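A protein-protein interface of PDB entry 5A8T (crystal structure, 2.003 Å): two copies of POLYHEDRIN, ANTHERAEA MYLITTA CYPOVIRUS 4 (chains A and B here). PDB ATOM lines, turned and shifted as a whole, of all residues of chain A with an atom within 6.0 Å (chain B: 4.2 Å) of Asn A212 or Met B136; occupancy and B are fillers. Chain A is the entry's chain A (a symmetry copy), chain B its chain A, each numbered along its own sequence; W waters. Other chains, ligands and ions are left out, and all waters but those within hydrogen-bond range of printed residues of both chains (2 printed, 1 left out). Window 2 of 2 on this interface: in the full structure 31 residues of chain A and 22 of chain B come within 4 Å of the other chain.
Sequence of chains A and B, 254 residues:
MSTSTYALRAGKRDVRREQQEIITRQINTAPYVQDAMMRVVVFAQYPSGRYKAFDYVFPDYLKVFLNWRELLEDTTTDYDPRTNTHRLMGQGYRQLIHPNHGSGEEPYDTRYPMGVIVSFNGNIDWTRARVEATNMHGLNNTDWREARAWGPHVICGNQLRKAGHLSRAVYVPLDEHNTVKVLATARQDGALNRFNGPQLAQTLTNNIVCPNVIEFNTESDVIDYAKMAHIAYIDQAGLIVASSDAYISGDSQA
The backbone carbonyl oxygen (O) of Met B136 sits at hydrogen-bond distance from the side-chain amide nitrogen (ND2) of Asn A212 (2.7 Å).
The side-chain amide oxygen of Asn B135 lies within hydrogen-bond range of the backbone NH of His B137, 2.9 Å away. The side-chain amide oxygen (OD1) of Asn B135 is in hydrogen-bond range of the backbone NH (N) of Gly B138, 3.3 Å away. The backbone NH (N) of Met B136 sits at hydrogen-bond distance from the backbone carbonyl oxygen (O) of His B177, 3.2 Å away. The backbone carbonyl oxygen (O) of Asn A212 is in hydrogen-bond range of the backbone NH (N) of Asp A55, 2.8 Å away.
Among the printed residues, pairs that only touch across the chains: Cys A210 with His B137 (3.8 Å), Cys A210 with Gly B138 (3.99 Å), Asn A212 with Trp B68 (3.6 Å) and Asn A212 with His B137 (3.4 Å).
Of the printed residues of chain B, Asn A212 touches Trp B68, Met B136 and His B137. Met B136 touches just one residue of chain A: Asn A212 (2.7 Å). Of the printed residues of chain A, Trp B68 touches Asn A212 (3.6 Å). Printed residues of chain A within 4 Å of Gly B138: Cys A210. Printed residues of chain B within 4 Å of Cys A210: His B137 (3.8 Å) and Gly B138 (3.99 Å). Of the printed residues of chain A, His B137 touches Cys A210 and Asn A212. Asn B135 touches none of the printed residues of chain A. The nearest printed residue of chain B that does not touch Asn A212 is Gly B138 (4.5 Å). The nearest printed residue of chain A that does not touch Met B136 is Pro A211 (6.1 Å).
Printed residues of chain B that touch a printed residue of chain A: Trp B68, Met B136, His B137 and Gly B138. Hydrophobic or aromatic side chains of chain B that line the printed part of chain A: Trp B68. Along chain B the printed residues that touch a printed residue of chain A span positions 68 to 138. Among the printed residues, 5 pairs touch across the chains. Among the printed residues, no Asp or Glu carboxylate lies within 4 Å of a Lys or Arg side-chain nitrogen of the other chain.
No position is printed for both chains. Of the 5 pairs that touch across the chains among the printed residues, none has its exchanged pair printed and touching as well.
Water W2 lies within hydrogen-bond range of O of Gly B138 (2.5 Å) and SG of Cys A210 (3.6 Å). Water W1 lies within hydrogen-bond range of N of Trp B68, O of Met B136 and OD1 of Asn A212.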
ATOM      1  N   ALA A  53      26.360   0.009 -22.186  1.00  0.00           N
ATOM      2  CA  ALA A  53      26.229  -1.378 -22.605  1.00  0.00           C
ATOM      3  C   ALA A  53      25.985  -1.444 -24.100  1.00  0.00           C
ATOM      4  O   ALA A  53      25.174  -0.690 -24.632  1.00  0.00           O
ATOM      5  CB  ALA A  53      25.098  -2.067 -21.849  1.00  0.00           C
ATOM      6  N   PHE A  54      26.729  -2.313 -24.778  1.00  0.00           N
ATOM      7  CA  PHE A  54      26.465  -2.633 -26.175  1.00  0.00           C
ATOM      8  C   PHE A  54      25.773  -3.983 -26.194  1.00  0.00           C
ATOM      9  O   PHE A  54      26.387  -5.014 -25.974  1.00  0.00           O
ATOM     10  CB  PHE A  54      27.750  -2.641 -27.001  1.00  0.00           C
ATOM     11  CG  PHE A  54      28.482  -1.334 -26.974  1.00  0.00           C
ATOM     12  CD1 PHE A  54      29.401  -1.056 -25.972  1.00  0.00           C
ATOM     13  CD2 PHE A  54      28.237  -0.370 -27.937  1.00  0.00           C
ATOM     14  CE1 PHE A  54      30.065   0.162 -25.935  1.00  0.00           C
ATOM     15  CE2 PHE A  54      28.894   0.846 -27.905  1.00  0.00           C
ATOM     16  CZ  PHE A  54      29.808   1.111 -26.906  1.00  0.00           C
ATOM     17  N   ASP A  55      24.466  -3.948 -26.415  1.00  0.00           N
ATOM     18  CA  ASP A  55      23.603  -5.103 -26.215  1.00  0.00           C
ATOM     19  C   ASP A  55      23.164  -5.669 -27.564  1.00  0.00           C
ATOM     20  O   ASP A  55      22.450  -5.006 -28.326  1.00  0.00           O
ATOM     21  CB  ASP A  55      22.384  -4.667 -25.400  1.00  0.00           C
ATOM     22  CG  ASP A  55      21.538  -5.830 -24.938  1.00  0.00           C
ATOM     23  OD1 ASP A  55      21.754  -6.967 -25.401  1.00  0.00           O
ATOM     24  OD2 ASP A  55      20.637  -5.597 -24.107  1.00  0.00           O
ATOM     25  N   TYR A  56      23.607  -6.883 -27.872  1.00  0.00           N
ATOM     26  CA  TYR A  56      23.284  -7.488 -29.163  1.00  0.00           C
ATOM     27  C   TYR A  56      22.408  -8.716 -28.994  1.00  0.00           C
ATOM     28  O   TYR A  56      22.736  -9.601 -28.214  1.00  0.00           O
ATOM     29  CB  TYR A  56      24.554  -7.917 -29.896  1.00  0.00           C
ATOM     30  CG  TYR A  56      25.580  -6.837 -30.040  1.00  0.00           C
ATOM     31  CD1 TYR A  56      26.498  -6.597 -29.025  1.00  0.00           C
ATOM     32  CD2 TYR A  56      25.637  -6.048 -31.186  1.00  0.00           C
ATOM     33  CE1 TYR A  56      27.457  -5.612 -29.143  1.00  0.00           C
ATOM     34  CE2 TYR A  56      26.595  -5.046 -31.310  1.00  0.00           C
ATOM     35  CZ  TYR A  56      27.501  -4.837 -30.280  1.00  0.00           C
ATOM     36  OH  TYR A  56      28.464  -3.859 -30.370  1.00  0.00           O
ATOM     37  N   CYS A 210      20.664  -7.334 -33.868  1.00  0.00           N
ATOM     38  CA  CYS A 210      19.911  -6.173 -33.405  1.00  0.00           C
ATOM     39  C   CYS A 210      20.632  -5.541 -32.234  1.00  0.00           C
ATOM     40  O   CYS A 210      20.488  -6.006 -31.105  1.00  0.00           O
ATOM     41  CB  CYS A 210      18.509  -6.604 -32.964  1.00  0.00           C
ATOM     42  SG  CYS A 210      17.589  -7.461 -34.253  1.00  0.00           S
ATOM     43  N   PRO A 211      21.424  -4.486 -32.498  1.00  0.00           N
ATOM     44  CA  PRO A 211      22.232  -3.833 -31.464  1.00  0.00           C
ATOM     45  C   PRO A 211      21.503  -2.683 -30.799  1.00  0.00           C
ATOM     46  O   PRO A 211      20.789  -1.934 -31.463  1.00  0.00           O
ATOM     47  CB  PRO A 211      23.428  -3.267 -32.251  1.00  0.00           C
ATOM     48  CG  PRO A 211      23.054  -3.388 -33.728  1.00  0.00           C
ATOM     49  CD  PRO A 211      21.627  -3.853 -33.811  1.00  0.00           C
ATOM     50  N   ASN A 212      21.669  -2.563 -29.490  1.00  0.00           N
ATOM     51  CA  ASN A 212      21.249  -1.370 -28.779  1.00  0.00           C
ATOM     52  C   ASN A 212      22.348  -0.876 -27.873  1.00  0.00           C
ATOM     53  O   ASN A 212      23.054  -1.674 -27.254  1.00  0.00           O
ATOM     54  CB  ASN A 212      19.963  -1.607 -27.992  1.00  0.00           C
ATOM     55  CG  ASN A 212      18.732  -1.330 -28.824  1.00  0.00           C
ATOM     56  OD1 ASN A 212      18.490  -0.186 -29.226  1.00  0.00           O
ATOM     57  ND2 ASN A 212      17.954  -2.374 -29.109  1.00  0.00           N
ATOM     58  N   VAL A 213      22.519   0.440 -27.824  1.00  0.00           N
ATOM     59  CA  VAL A 213      23.442   1.040 -26.871  1.00  0.00           C
ATOM     60  C   VAL A 213      22.625   1.660 -25.745  1.00  0.00           C
ATOM     61  O   VAL A 213      21.644   2.374 -25.988  1.00  0.00           O
ATOM     62  CB  VAL A 213      24.357   2.089 -27.516  1.00  0.00           C
ATOM     63  CG1 VAL A 213      25.309   2.684 -26.472  1.00  0.00           C
ATOM     64  CG2 VAL A 213      25.146   1.465 -28.641  1.00  0.00           C
ATOM     65  N   ILE A 214      23.019   1.355 -24.512  1.00  0.00           N
ATOM     66  CA  ILE A 214      22.279   1.792 -23.334  1.00  0.00           C
ATOM     67  C   ILE A 214      23.227   2.421 -22.319  1.00  0.00           C
ATOM     68  O   ILE A 214      24.262   1.846 -21.979  1.00  0.00           O
ATOM     69  CB  ILE A 214      21.539   0.610 -22.682  1.00  0.00           C
ATOM     70  CG1 ILE A 214      20.676  -0.108 -23.723  1.00  0.00           C
ATOM     71  CG2 ILE A 214      20.683   1.087 -21.512  1.00  0.00           C
ATOM     72  CD1 ILE A 214      20.570  -1.593 -23.504  1.00  0.00           C
ATOM     73  N   TRP B  68      15.115   2.077 -32.514  1.00  0.00           N
ATOM     74  CA  TRP B  68      14.172   3.127 -32.152  1.00  0.00           C
ATOM     75  C   TRP B  68      14.749   4.510 -32.411  1.00  0.00           C
ATOM     76  O   TRP B  68      14.020   5.427 -32.768  1.00  0.00           O
ATOM     77  CB  TRP B  68      13.735   2.991 -30.689  1.00  0.00           C
ATOM     78  CG  TRP B  68      14.863   3.148 -29.721  1.00  0.00           C
ATOM     79  CD1 TRP B  68      15.629   2.150 -29.178  1.00  0.00           C
ATOM     80  CD2 TRP B  68      15.370   4.377 -29.189  1.00  0.00           C
ATOM     81  NE1 TRP B  68      16.580   2.687 -28.339  1.00  0.00           N
ATOM     82  CE2 TRP B  68      16.441   4.051 -28.328  1.00  0.00           C
ATOM     83  CE3 TRP B  68      15.024   5.723 -29.358  1.00  0.00           C
ATOM     84  CZ2 TRP B  68      17.164   5.021 -27.635  1.00  0.00           C
ATOM     85  CZ3 TRP B  68      15.742   6.685 -28.668  1.00  0.00           C
ATOM     86  CH2 TRP B  68      16.800   6.330 -27.816  1.00  0.00           C
ATOM     87  N   ASN B 135      10.201  -5.369 -30.268  1.00  0.00           N
ATOM     88  CA  ASN B 135      10.267  -4.365 -29.206  1.00  0.00           C
ATOM     89  C   ASN B 135      11.523  -3.510 -29.333  1.00  0.00           C
ATOM     90  O   ASN B 135      12.212  -3.567 -30.350  1.00  0.00           O
ATOM     91  CB  ASN B 135      10.107  -4.981 -27.805  1.00  0.00           C
ATOM     92  CG  ASN B 135      11.300  -5.811 -27.375  1.00  0.00           C
ATOM     93  OD1 ASN B 135      12.325  -5.883 -28.064  1.00  0.00           O
ATOM     94  ND2 ASN B 135      11.173  -6.447 -26.214  1.00  0.00           N
ATOM     95  N   MET B 136      11.821  -2.706 -28.321  1.00  0.00           N
ATOM     96  CA  MET B 136      12.941  -1.773 -28.441  1.00  0.00           C
ATOM     97  C   MET B 136      14.294  -2.477 -28.487  1.00  0.00           C
ATOM     98  O   MET B 136      15.299  -1.877 -28.864  1.00  0.00           O
ATOM     99  CB  MET B 136      12.918  -0.743 -27.314  1.00  0.00           C
ATOM    100  CG  MET B 136      12.670  -1.341 -25.946  1.00  0.00           C
ATOM    101  SD  MET B 136      12.740  -0.103 -24.633  1.00  0.00           S
ATOM    102  CE  MET B 136      12.355  -1.107 -23.198  1.00  0.00           C
ATOM    103  N   HIS B 137      14.314  -3.753 -28.119  1.00  0.00           N
ATOM    104  CA  HIS B 137      15.555  -4.529 -28.124  1.00  0.00           C
ATOM    105  C   HIS B 137      15.705  -5.340 -29.408  1.00  0.00           C
ATOM    106  O   HIS B 137      16.710  -6.027 -29.612  1.00  0.00           O
ATOM    107  CB  HIS B 137      15.608  -5.455 -26.908  1.00  0.00           C
ATOM    108  CG  HIS B 137      15.710  -4.721 -25.608  1.00  0.00           C
ATOM    109  ND1 HIS B 137      14.603  -4.325 -24.887  1.00  0.00           N
ATOM    110  CD2 HIS B 137      16.789  -4.279 -24.917  1.00  0.00           C
ATOM    111  CE1 HIS B 137      14.995  -3.680 -23.801  1.00  0.00           C
ATOM    112  NE2 HIS B 137      16.317  -3.639 -23.795  1.00  0.00           N
ATOM    113  N   GLY B 138      14.703  -5.239 -30.274  1.00  0.00           N
ATOM    114  CA  GLY B 138      14.629  -6.075 -31.453  1.00  0.00           C
ATOM    115  C   GLY B 138      14.168  -7.495 -31.170  1.00  0.00           C
ATOM    116  O   GLY B 138      14.480  -8.413 -31.933  1.00  0.00           O
ATOM    117  N   HIS B 177       7.110   1.918 -28.764  1.00  0.00           N
ATOM    118  CA  HIS B 177       8.147   0.972 -28.366  1.00  0.00           C
ATOM    119  C   HIS B 177       8.579  -0.010 -29.468  1.00  0.00           C
ATOM    120  O   HIS B 177       9.171  -1.050 -29.171  1.00  0.00           O
ATOM    121  CB  HIS B 177       7.719   0.214 -27.098  1.00  0.00           C
ATOM    122  CG  HIS B 177       7.394  -1.233 -27.326  1.00  0.00           C
ATOM    123  ND1 HIS B 177       6.318  -1.647 -28.085  1.00  0.00           N
ATOM    124  CD2 HIS B 177       7.996  -2.362 -26.881  1.00  0.00           C
ATOM    125  CE1 HIS B 177       6.275  -2.968 -28.101  1.00  0.00           C
ATOM    126  NE2 HIS B 177       7.281  -3.427 -27.378  1.00  0.00           N
ATOM    127  N   THR B 179      10.536  -1.505 -32.960  1.00  0.00           N
ATOM    128  CA  THR B 179      11.610  -1.470 -33.936  1.00  0.00           C
ATOM    129  C   THR B 179      11.127  -2.226 -35.162  1.00  0.00           C
ATOM    130  O   THR B 179      10.076  -2.865 -35.120  1.00  0.00           O
ATOM    131  CB  THR B 179      12.910  -2.090 -33.395  1.00  0.00           C
ATOM    132  OG1 THR B 179      12.628  -3.356 -32.787  1.00  0.00           O
ATOM    133  CG2 THR B 179      13.536  -1.170 -32.356  1.00  0.00           C
HETATM  134  O   HOH W   1      16.104  -0.045 -30.918  1.00  0.00           O
HETATM  135  O   HOH W   2      14.995  -9.978 -33.750  1.00  0.00           O
